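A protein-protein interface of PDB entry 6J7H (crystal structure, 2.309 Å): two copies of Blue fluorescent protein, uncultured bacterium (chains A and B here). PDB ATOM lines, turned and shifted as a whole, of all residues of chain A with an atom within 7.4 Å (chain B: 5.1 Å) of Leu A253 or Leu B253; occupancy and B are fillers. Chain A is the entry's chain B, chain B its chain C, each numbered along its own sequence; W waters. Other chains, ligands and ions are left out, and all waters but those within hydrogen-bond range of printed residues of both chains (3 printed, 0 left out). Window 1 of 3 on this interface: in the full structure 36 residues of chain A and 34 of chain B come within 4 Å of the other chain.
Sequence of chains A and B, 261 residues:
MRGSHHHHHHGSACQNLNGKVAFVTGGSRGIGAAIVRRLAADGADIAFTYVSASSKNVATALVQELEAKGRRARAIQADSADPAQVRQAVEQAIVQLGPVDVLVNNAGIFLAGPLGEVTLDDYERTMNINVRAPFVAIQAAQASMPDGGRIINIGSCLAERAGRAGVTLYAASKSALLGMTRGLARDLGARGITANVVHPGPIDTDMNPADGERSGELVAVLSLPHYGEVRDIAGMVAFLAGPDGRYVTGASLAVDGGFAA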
ATOM      1  N   ILE A 152       0.260  33.592 -14.742  1.00  0.00           N
ATOM      2  CA  ILE A 152      -0.401  32.299 -14.565  1.00  0.00           C
ATOM      3  C   ILE A 152       0.543  31.395 -13.786  1.00  0.00           C
ATOM      4  O   ILE A 152       1.509  30.867 -14.346  1.00  0.00           O
ATOM      5  CB  ILE A 152      -0.779  31.656 -15.897  1.00  0.00           C
ATOM      6  CG1 ILE A 152      -1.654  32.606 -16.709  1.00  0.00           C
ATOM      7  CG2 ILE A 152      -1.467  30.320 -15.644  1.00  0.00           C
ATOM      8  CD1 ILE A 152      -1.835  32.183 -18.146  1.00  0.00           C
ATOM      9  N   ASN A 153       0.274  31.214 -12.502  1.00  0.00           N
ATOM     10  CA  ASN A 153       1.020  30.271 -11.689  1.00  0.00           C
ATOM     11  C   ASN A 153       0.428  28.879 -11.773  1.00  0.00           C
ATOM     12  O   ASN A 153      -0.792  28.695 -11.830  1.00  0.00           O
ATOM     13  CB  ASN A 153       1.051  30.762 -10.251  1.00  0.00           C
ATOM     14  CG  ASN A 153       1.718  32.109 -10.150  1.00  0.00           C
ATOM     15  OD1 ASN A 153       2.698  32.368 -10.862  1.00  0.00           O
ATOM     16  ND2 ASN A 153       1.176  32.993  -9.319  1.00  0.00           N
ATOM     17  N   GLU A 160      -5.008  22.753  -2.134  1.00  0.00           N
ATOM     18  CA  GLU A 160      -6.334  22.933  -1.540  1.00  0.00           C
ATOM     19  C   GLU A 160      -6.785  21.756  -0.691  1.00  0.00           C
ATOM     20  O   GLU A 160      -7.554  21.947   0.257  1.00  0.00           O
ATOM     21  CB  GLU A 160      -7.394  23.150  -2.627  1.00  0.00           C
ATOM     22  CG  GLU A 160      -7.172  24.354  -3.547  1.00  0.00           C
ATOM     23  CD  GLU A 160      -7.477  25.687  -2.884  1.00  0.00           C
ATOM     24  OE1 GLU A 160      -7.784  25.714  -1.673  1.00  0.00           O
ATOM     25  OE2 GLU A 160      -7.419  26.715  -3.586  1.00  0.00           O
ATOM     26  N   LEU A 178      -1.411  30.466  -3.540  1.00  0.00           N
ATOM     27  CA  LEU A 178      -2.786  30.951  -3.464  1.00  0.00           C
ATOM     28  C   LEU A 178      -2.827  32.406  -3.008  1.00  0.00           C
ATOM     29  O   LEU A 178      -3.427  33.262  -3.673  1.00  0.00           O
ATOM     30  CB  LEU A 178      -3.584  30.062  -2.506  1.00  0.00           C
ATOM     31  CG  LEU A 178      -3.899  28.675  -3.064  1.00  0.00           C
ATOM     32  CD1 LEU A 178      -4.599  27.809  -2.030  1.00  0.00           C
ATOM     33  CD2 LEU A 178      -4.736  28.803  -4.320  1.00  0.00           C
ATOM     34  N   ALA A 195      -3.938  37.827 -12.687  1.00  0.00           N
ATOM     35  CA  ALA A 195      -3.061  36.881 -12.009  1.00  0.00           C
ATOM     36  C   ALA A 195      -3.910  35.716 -11.522  1.00  0.00           C
ATOM     37  O   ALA A 195      -4.837  35.921 -10.736  1.00  0.00           O
ATOM     38  CB  ALA A 195      -2.329  37.554 -10.842  1.00  0.00           C
ATOM     39  N   ASN A 196      -3.597  34.500 -11.976  1.00  0.00           N
ATOM     40  CA  ASN A 196      -4.401  33.328 -11.638  1.00  0.00           C
ATOM     41  C   ASN A 196      -3.496  32.140 -11.347  1.00  0.00           C
ATOM     42  O   ASN A 196      -2.329  32.116 -11.741  1.00  0.00           O
ATOM     43  CB  ASN A 196      -5.397  32.972 -12.763  1.00  0.00           C
ATOM     44  CG  ASN A 196      -6.400  34.085 -13.039  1.00  0.00           C
ATOM     45  OD1 ASN A 196      -7.333  34.301 -12.258  1.00  0.00           O
ATOM     46  ND2 ASN A 196      -6.240  34.773 -14.170  1.00  0.00           N
ATOM     47  N   VAL A 197      -4.044  31.138 -10.659  1.00  0.00           N
ATOM     48  CA  VAL A 197      -3.334  29.889 -10.405  1.00  0.00           C
ATOM     49  C   VAL A 197      -4.177  28.705 -10.888  1.00  0.00           C
ATOM     50  O   VAL A 197      -5.379  28.624 -10.607  1.00  0.00           O
ATOM     51  CB  VAL A 197      -2.923  29.742  -8.918  1.00  0.00           C
ATOM     52  CG1 VAL A 197      -4.072  30.058  -7.959  1.00  0.00           C
ATOM     53  CG2 VAL A 197      -2.303  28.349  -8.640  1.00  0.00           C
ATOM     54  N   VAL A 198      -3.546  27.819 -11.672  1.00  0.00           N
ATOM     55  CA  VAL A 198      -4.145  26.588 -12.191  1.00  0.00           C
ATOM     56  C   VAL A 198      -3.642  25.419 -11.358  1.00  0.00           C
ATOM     57  O   VAL A 198      -2.425  25.264 -11.161  1.00  0.00           O
ATOM     58  CB  VAL A 198      -3.794  26.399 -13.683  1.00  0.00           C
ATOM     59  CG1 VAL A 198      -4.316  25.094 -14.222  1.00  0.00           C
ATOM     60  CG2 VAL A 198      -4.329  27.556 -14.506  1.00  0.00           C
ATOM     61  N   HIS A 199      -4.563  24.530 -10.963  1.00  0.00           N
ATOM     62  CA  HIS A 199      -4.251  23.421 -10.065  1.00  0.00           C
ATOM     63  C   HIS A 199      -4.417  22.106 -10.798  1.00  0.00           C
ATOM     64  O   HIS A 199      -5.550  21.624 -10.959  1.00  0.00           O
ATOM     65  CB  HIS A 199      -5.159  23.435  -8.833  1.00  0.00           C
ATOM     66  CG  HIS A 199      -4.913  24.566  -7.895  1.00  0.00           C
ATOM     67  ND1 HIS A 199      -3.666  24.851  -7.381  1.00  0.00           N
ATOM     68  CD2 HIS A 199      -5.768  25.452  -7.329  1.00  0.00           C
ATOM     69  CE1 HIS A 199      -3.759  25.884  -6.562  1.00  0.00           C
ATOM     70  NE2 HIS A 199      -5.025  26.260  -6.507  1.00  0.00           N
ATOM     71  N   PRO A 200      -3.344  21.514 -11.307  1.00  0.00           N
ATOM     72  CA  PRO A 200      -3.460  20.176 -11.900  1.00  0.00           C
ATOM     73  C   PRO A 200      -3.834  19.120 -10.868  1.00  0.00           C
ATOM     74  O   PRO A 200      -3.376  19.146  -9.723  1.00  0.00           O
ATOM     75  CB  PRO A 200      -2.065  19.927 -12.490  1.00  0.00           C
ATOM     76  CG  PRO A 200      -1.445  21.326 -12.635  1.00  0.00           C
ATOM     77  CD  PRO A 200      -1.989  22.082 -11.450  1.00  0.00           C
ATOM     78  N   ILE A 233      -3.934  20.850 -19.083  1.00  0.00           N
ATOM     79  CA  ILE A 233      -3.358  22.004 -18.404  1.00  0.00           C
ATOM     80  C   ILE A 233      -3.048  23.106 -19.408  1.00  0.00           C
ATOM     81  O   ILE A 233      -3.302  24.285 -19.147  1.00  0.00           O
ATOM     82  CB  ILE A 233      -2.115  21.583 -17.599  1.00  0.00           C
ATOM     83  CG1 ILE A 233      -2.461  20.406 -16.684  1.00  0.00           C
ATOM     84  CG2 ILE A 233      -1.580  22.752 -16.787  1.00  0.00           C
ATOM     85  CD1 ILE A 233      -3.693  20.643 -15.785  1.00  0.00           C
ATOM     86  N   MET A 236      -6.145  25.166 -20.392  1.00  0.00           N
ATOM     87  CA  MET A 236      -6.534  26.123 -19.363  1.00  0.00           C
ATOM     88  C   MET A 236      -5.621  27.340 -19.364  1.00  0.00           C
ATOM     89  O   MET A 236      -6.092  28.476 -19.240  1.00  0.00           O
ATOM     90  CB  MET A 236      -6.525  25.459 -17.982  1.00  0.00           C
ATOM     91  CG  MET A 236      -6.793  26.453 -16.856  1.00  0.00           C
ATOM     92  SD  MET A 236      -8.421  27.255 -16.965  1.00  0.00           S
ATOM     93  CE  MET A 236      -9.496  25.988 -16.271  1.00  0.00           C
ATOM     94  N   PHE A 239      -6.483  29.488 -22.324  1.00  0.00           N
ATOM     95  CA  PHE A 239      -7.702  30.252 -22.102  1.00  0.00           C
ATOM     96  C   PHE A 239      -7.414  31.498 -21.275  1.00  0.00           C
ATOM     97  O   PHE A 239      -7.884  32.597 -21.592  1.00  0.00           O
ATOM     98  CB  PHE A 239      -8.741  29.370 -21.396  1.00  0.00           C
ATOM     99  CG  PHE A 239      -9.920  30.132 -20.872  1.00  0.00           C
ATOM    100  CD1 PHE A 239     -10.995  30.417 -21.695  1.00  0.00           C
ATOM    101  CD2 PHE A 239      -9.933  30.601 -19.572  1.00  0.00           C
ATOM    102  CE1 PHE A 239     -12.077  31.132 -21.219  1.00  0.00           C
ATOM    103  CE2 PHE A 239     -11.011  31.322 -19.090  1.00  0.00           C
ATOM    104  CZ  PHE A 239     -12.083  31.590 -19.920  1.00  0.00           C
ATOM    105  N   LEU A 240      -6.653  31.338 -20.192  1.00  0.00           N
ATOM    106  CA  LEU A 240      -6.334  32.478 -19.338  1.00  0.00           C
ATOM    107  C   LEU A 240      -5.450  33.494 -20.046  1.00  0.00           C
ATOM    108  O   LEU A 240      -5.552  34.695 -19.761  1.00  0.00           O
ATOM    109  CB  LEU A 240      -5.662  31.996 -18.057  1.00  0.00           C
ATOM    110  CG  LEU A 240      -6.502  31.115 -17.134  1.00  0.00           C
ATOM    111  CD1 LEU A 240      -5.617  30.607 -16.019  1.00  0.00           C
ATOM    112  CD2 LEU A 240      -7.694  31.880 -16.563  1.00  0.00           C
ATOM    113  N   VAL A 248     -10.965  37.305 -15.769  1.00  0.00           N
ATOM    114  CA  VAL A 248     -10.653  36.295 -14.753  1.00  0.00           C
ATOM    115  C   VAL A 248      -9.350  36.693 -14.068  1.00  0.00           C
ATOM    116  O   VAL A 248      -8.282  36.676 -14.693  1.00  0.00           O
ATOM    117  CB  VAL A 248     -10.531  34.889 -15.361  1.00  0.00           C
ATOM    118  CG1 VAL A 248     -10.197  33.868 -14.273  1.00  0.00           C
ATOM    119  CG2 VAL A 248     -11.812  34.493 -16.106  1.00  0.00           C
ATOM    120  N   THR A 249      -9.411  37.014 -12.773  1.00  0.00           N
ATOM    121  CA  THR A 249      -8.197  37.358 -12.039  1.00  0.00           C
ATOM    122  C   THR A 249      -8.374  37.040 -10.557  1.00  0.00           C
ATOM    123  O   THR A 249      -9.475  37.149 -10.013  1.00  0.00           O
ATOM    124  CB  THR A 249      -7.832  38.834 -12.254  1.00  0.00           C
ATOM    125  OG1 THR A 249      -6.570  39.120 -11.640  1.00  0.00           O
ATOM    126  CG2 THR A 249      -8.900  39.744 -11.678  1.00  0.00           C
ATOM    127  N   GLY A 250      -7.295  36.598  -9.918  1.00  0.00           N
ATOM    128  CA  GLY A 250      -7.351  36.241  -8.521  1.00  0.00           C
ATOM    129  C   GLY A 250      -7.984  34.893  -8.245  1.00  0.00           C
ATOM    130  O   GLY A 250      -8.182  34.549  -7.072  1.00  0.00           O
ATOM    131  N   ALA A 251      -8.277  34.114  -9.284  1.00  0.00           N
ATOM    132  CA  ALA A 251      -9.005  32.859  -9.164  1.00  0.00           C
ATOM    133  C   ALA A 251      -8.066  31.662  -9.057  1.00  0.00           C
ATOM    134  O   ALA A 251      -6.937  31.681  -9.560  1.00  0.00           O
ATOM    135  CB  ALA A 251      -9.938  32.675 -10.366  1.00  0.00           C
ATOM    136  N   SER A 252      -8.547  30.616  -8.388  1.00  0.00           N
ATOM    137  CA  SER A 252      -7.902  29.306  -8.392  1.00  0.00           C
ATOM    138  C   SER A 252      -8.734  28.378  -9.265  1.00  0.00           C
ATOM    139  O   SER A 252      -9.913  28.141  -8.972  1.00  0.00           O
ATOM    140  CB  SER A 252      -7.780  28.730  -6.984  1.00  0.00           C
ATOM    141  OG  SER A 252      -7.073  29.611  -6.146  1.00  0.00           O
ATOM    142  N   LEU A 253      -8.119  27.837 -10.309  1.00  0.00           N
ATOM    143  CA  LEU A 253      -8.827  27.067 -11.328  1.00  0.00           C
ATOM    144  C   LEU A 253      -8.314  25.628 -11.308  1.00  0.00           C
ATOM    145  O   LEU A 253      -7.238  25.340 -11.846  1.00  0.00           O
ATOM    146  CB  LEU A 253      -8.618  27.717 -12.689  1.00  0.00           C
ATOM    147  CG  LEU A 253      -9.143  29.157 -12.679  1.00  0.00           C
ATOM    148  CD1 LEU A 253      -8.119  30.111 -13.261  1.00  0.00           C
ATOM    149  CD2 LEU A 253     -10.436  29.263 -13.417  1.00  0.00           C
ATOM    150  N   ALA A 254      -9.089  24.727 -10.696  1.00  0.00           N
ATOM    151  CA  ALA A 254      -8.725  23.316 -10.679  1.00  0.00           C
ATOM    152  C   ALA A 254      -8.956  22.671 -12.041  1.00  0.00           C
ATOM    153  O   ALA A 254     -10.005  22.853 -12.661  1.00  0.00           O
ATOM    154  CB  ALA A 254      -9.530  22.575  -9.608  1.00  0.00           C
ATOM    155  N   VAL A 255      -7.994  21.850 -12.464  1.00  0.00           N
ATOM    156  CA  VAL A 255      -8.117  20.944 -13.606  1.00  0.00           C
ATOM    157  C   VAL A 255      -7.729  19.572 -13.063  1.00  0.00           C
ATOM    158  O   VAL A 255      -6.661  19.035 -13.385  1.00  0.00           O
ATOM    159  CB  VAL A 255      -7.224  21.363 -14.799  1.00  0.00           C
ATOM    160  CG1 VAL A 255      -7.522  20.517 -16.021  1.00  0.00           C
ATOM    161  CG2 VAL A 255      -7.401  22.850 -15.134  1.00  0.00           C
ATOM    162  N   ASP A 256      -8.563  19.032 -12.170  1.00  0.00           N
ATOM    163  CA  ASP A 256      -8.172  17.927 -11.302  1.00  0.00           C
ATOM    164  C   ASP A 256      -9.014  16.666 -11.468  1.00  0.00           C
ATOM    165  O   ASP A 256      -8.896  15.754 -10.638  1.00  0.00           O
ATOM    166  CB  ASP A 256      -8.219  18.381  -9.839  1.00  0.00           C
ATOM    167  CG  ASP A 256      -9.628  18.733  -9.370  1.00  0.00           C
ATOM    168  OD1 ASP A 256     -10.557  18.780 -10.207  1.00  0.00           O
ATOM    169  OD2 ASP A 256      -9.808  18.953  -8.152  1.00  0.00           O
ATOM    170  N   ASN B 196     -19.757  21.994 -13.559  1.00  0.00           N
ATOM    171  CA  ASN B 196     -19.019  23.139 -13.040  1.00  0.00           C
ATOM    172  C   ASN B 196     -19.991  24.290 -12.826  1.00  0.00           C
ATOM    173  O   ASN B 196     -21.069  24.323 -13.406  1.00  0.00           O
ATOM    174  CB  ASN B 196     -17.871  23.558 -14.000  1.00  0.00           C
ATOM    175  CG  ASN B 196     -16.817  22.459 -14.178  1.00  0.00           C
ATOM    176  OD1 ASN B 196     -15.982  22.252 -13.299  1.00  0.00           O
ATOM    177  ND2 ASN B 196     -16.850  21.761 -15.323  1.00  0.00           N
ATOM    178  N   VAL B 197     -19.605  25.249 -11.997  1.00  0.00           N
ATOM    179  CA  VAL B 197     -20.408  26.449 -11.795  1.00  0.00           C
ATOM    180  C   VAL B 197     -19.532  27.670 -12.071  1.00  0.00           C
ATOM    181  O   VAL B 197     -18.375  27.726 -11.642  1.00  0.00           O
ATOM    182  CB  VAL B 197     -21.060  26.483 -10.385  1.00  0.00           C
ATOM    183  CG1 VAL B 197     -20.069  26.142  -9.280  1.00  0.00           C
ATOM    184  CG2 VAL B 197     -21.716  27.832 -10.110  1.00  0.00           C
ATOM    185  N   VAL B 198     -20.052  28.596 -12.877  1.00  0.00           N
ATOM    186  CA  VAL B 198     -19.383  29.851 -13.205  1.00  0.00           C
ATOM    187  C   VAL B 198     -19.995  30.967 -12.368  1.00  0.00           C
ATOM    188  O   VAL B 198     -21.229  31.104 -12.297  1.00  0.00           O
ATOM    189  CB  VAL B 198     -19.508  30.150 -14.712  1.00  0.00           C
ATOM    190  CG1 VAL B 198     -18.840  31.481 -15.073  1.00  0.00           C
ATOM    191  CG2 VAL B 198     -18.932  29.013 -15.517  1.00  0.00           C
ATOM    192  N   HIS B 199     -19.142  31.813 -11.792  1.00  0.00           N
ATOM    193  CA  HIS B 199     -19.597  32.860 -10.882  1.00  0.00           C
ATOM    194  C   HIS B 199     -19.320  34.200 -11.552  1.00  0.00           C
ATOM    195  O   HIS B 199     -18.172  34.681 -11.529  1.00  0.00           O
ATOM    196  CB  HIS B 199     -18.858  32.780  -9.540  1.00  0.00           C
ATOM    197  CG  HIS B 199     -19.141  31.547  -8.732  1.00  0.00           C
ATOM    198  ND1 HIS B 199     -20.418  31.146  -8.383  1.00  0.00           N
ATOM    199  CD2 HIS B 199     -18.300  30.639  -8.180  1.00  0.00           C
ATOM    200  CE1 HIS B 199     -20.347  30.045  -7.654  1.00  0.00           C
ATOM    201  NE2 HIS B 199     -19.074  29.717  -7.516  1.00  0.00           N
ATOM    202  N   MET B 236     -16.180  31.857 -20.887  1.00  0.00           N
ATOM    203  CA  MET B 236     -15.916  30.815 -19.902  1.00  0.00           C
ATOM    204  C   MET B 236     -16.800  29.597 -20.145  1.00  0.00           C
ATOM    205  O   MET B 236     -16.325  28.456 -20.118  1.00  0.00           O
ATOM    206  CB  MET B 236     -16.133  31.362 -18.489  1.00  0.00           C
ATOM    207  CG  MET B 236     -15.996  30.323 -17.385  1.00  0.00           C
ATOM    208  SD  MET B 236     -14.366  29.539 -17.320  1.00  0.00           S
ATOM    209  CE  MET B 236     -13.373  30.798 -16.511  1.00  0.00           C
ATOM    210  N   LEU B 240     -15.707  25.676 -20.952  1.00  0.00           N
ATOM    211  CA  LEU B 240     -16.130  24.461 -20.258  1.00  0.00           C
ATOM    212  C   LEU B 240     -16.882  23.511 -21.185  1.00  0.00           C
ATOM    213  O   LEU B 240     -16.836  22.291 -20.994  1.00  0.00           O
ATOM    214  CB  LEU B 240     -17.004  24.827 -19.058  1.00  0.00           C
ATOM    215  CG  LEU B 240     -16.336  25.652 -17.953  1.00  0.00           C
ATOM    216  CD1 LEU B 240     -17.384  26.054 -16.948  1.00  0.00           C
ATOM    217  CD2 LEU B 240     -15.184  24.901 -17.272  1.00  0.00           C
ATOM    218  N   VAL B 248     -12.080  19.291 -16.480  1.00  0.00           N
ATOM    219  CA  VAL B 248     -12.533  20.248 -15.472  1.00  0.00           C
ATOM    220  C   VAL B 248     -13.902  19.800 -14.960  1.00  0.00           C
ATOM    221  O   VAL B 248     -14.892  19.824 -15.701  1.00  0.00           O
ATOM    222  CB  VAL B 248     -12.605  21.665 -16.054  1.00  0.00           C
ATOM    223  CG1 VAL B 248     -13.082  22.676 -15.008  1.00  0.00           C
ATOM    224  CG2 VAL B 248     -11.257  22.066 -16.668  1.00  0.00           C
ATOM    225  N   ALA B 251     -15.642  22.116 -10.231  1.00  0.00           N
ATOM    226  CA  ALA B 251     -14.927  23.342  -9.915  1.00  0.00           C
ATOM    227  C   ALA B 251     -15.869  24.540  -9.894  1.00  0.00           C
ATOM    228  O   ALA B 251     -16.894  24.564 -10.582  1.00  0.00           O
ATOM    229  CB  ALA B 251     -13.791  23.582 -10.918  1.00  0.00           C
ATOM    230  N   SER B 252     -15.511  25.529  -9.080  1.00  0.00           N
ATOM    231  CA  SER B 252     -16.136  26.846  -9.091  1.00  0.00           C
ATOM    232  C   SER B 252     -15.137  27.812  -9.712  1.00  0.00           C
ATOM    233  O   SER B 252     -14.011  27.941  -9.214  1.00  0.00           O
ATOM    234  CB  SER B 252     -16.518  27.293  -7.680  1.00  0.00           C
ATOM    235  OG  SER B 252     -17.366  26.346  -7.059  1.00  0.00           O
ATOM    236  N   LEU B 253     -15.534  28.461 -10.808  1.00  0.00           N
ATOM    237  CA  LEU B 253     -14.651  29.304 -11.612  1.00  0.00           C
ATOM    238  C   LEU B 253     -15.169  30.736 -11.591  1.00  0.00           C
ATOM    239  O   LEU B 253     -16.201  31.033 -12.200  1.00  0.00           O
ATOM    240  CB  LEU B 253     -14.561  28.789 -13.047  1.00  0.00           C
ATOM    241  CG  LEU B 253     -13.951  27.402 -13.245  1.00  0.00           C
ATOM    242  CD1 LEU B 253     -14.981  26.302 -13.030  1.00  0.00           C
ATOM    243  CD2 LEU B 253     -13.361  27.297 -14.649  1.00  0.00           C
ATOM    244  N   ALA B 254     -14.492  31.611 -10.858  1.00  0.00           N
ATOM    245  CA  ALA B 254     -14.886  33.013 -10.841  1.00  0.00           C
ATOM    246  C   ALA B 254     -14.496  33.717 -12.136  1.00  0.00           C
ATOM    247  O   ALA B 254     -13.393  33.529 -12.660  1.00  0.00           O
ATOM    248  CB  ALA B 254     -14.267  33.726  -9.641  1.00  0.00           C
ATOM    249  N   VAL B 255     -15.410  34.555 -12.628  1.00  0.00           N
ATOM    250  CA  VAL B 255     -15.186  35.518 -13.702  1.00  0.00           C
ATOM    251  C   VAL B 255     -15.658  36.855 -13.146  1.00  0.00           C
ATOM    252  O   VAL B 255     -16.683  37.398 -13.574  1.00  0.00           O
ATOM    253  CB  VAL B 255     -15.941  35.141 -14.993  1.00  0.00           C
ATOM    254  CG1 VAL B 255     -15.509  36.036 -16.145  1.00  0.00           C
ATOM    255  CG2 VAL B 255     -15.721  33.666 -15.346  1.00  0.00           C
HETATM  256  O   HOH W   1     -12.579  30.366  -9.200  1.00  0.00           O
HETATM  257  O   HOH W   2     -12.419  36.265 -11.686  1.00  0.00           O
HETATM  258  O   HOH W   3     -11.488  25.894  -9.244  1.00  0.00           O
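ND2 of Asn A196 sits at hydrogen-bond distance from O of Val A248 (2.8 Å). O of Val A197 lies within hydrogen-bond range of N of Leu A253 (2.9 Å). The backbone NH (N) of His A199 lies within hydrogen-bond range of the backbone carbonyl oxygen (O) of Leu A253 (2.9 Å). The backbone carbonyl oxygen (O) of Val B248 is in hydrogen-bond range of the side-chain amide nitrogen (ND2) of Asn B196 (2.8 Å). O of Val B197 sits at hydrogen-bond distance from N of Leu B253, 3.1 Å away. The backbone carbonyl oxygen of Leu B253 lies within hydrogen-bond range of the backbone NH of His B199 (3.1 Å).
Among the printed residues, pairs that only touch across the chains: Phe A239 with Met B236, Val A248 with Ala B254, Leu A253 with Leu B253 and Ala A254 with Val B248.
Printed residues of chain B within 4 Å of Phe A239: Met B236. Printed residues of chain B within 4 Å of Val A248: Ala B254. Of chain B, only Leu B253 comes within 4 Å of Leu A253. Of the printed residues of chain B, Ala A254 touches Val B248 (3.9 Å). Of the printed residues of chain A, Val B248 touches Ala A254 (3.9 Å). Leu B253 touches just one residue of chain A: Leu A253 (3.7 Å). Of the printed residues of chain A, Ala B254 touches Val A248 (3.6 Å). The nearest residue of chain A that does not touch Leu B253 is Met A236 (4.4 Å).
Of the 23 printed residues of chain A, 4 touch a printed residue of chain B. Printed residues of chain A that touch a printed residue of chain B: Phe A239, Val A248, Leu A253 and Ala A254. Hydrophobic or aromatic side chains of chain A within 4 Å of the printed part of chain B: Phe A239, Val A248 and Leu A253. Along chain A the printed residues that touch a printed residue of chain B span positions 239 to 254. Among the printed residues, 4 pairs touch across the chains.
Val A248 touches Ala B254, and with the chains exchanged Ala A254 touches Val B248. Leu A253 touches its own counterpart, Leu B253. Of the 4 pairs that touch across the chains among the printed residues, 3 have their exchanged pair printed and touching as well.
Water W3 lies within hydrogen-bond range of O of Ser A252 (2.8 Å), N of Ala A254 (3.0 Å) and O of Ser B252 (3.2 Å). Water W1 lies within hydrogen-bond range of O of Ser B252, N of Ala B254 and O of Ser A252. Water W2 lies within hydrogen-bond range of O of Ala B254 (3.1 Å) and N of Thr A249 (3.3 Å).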
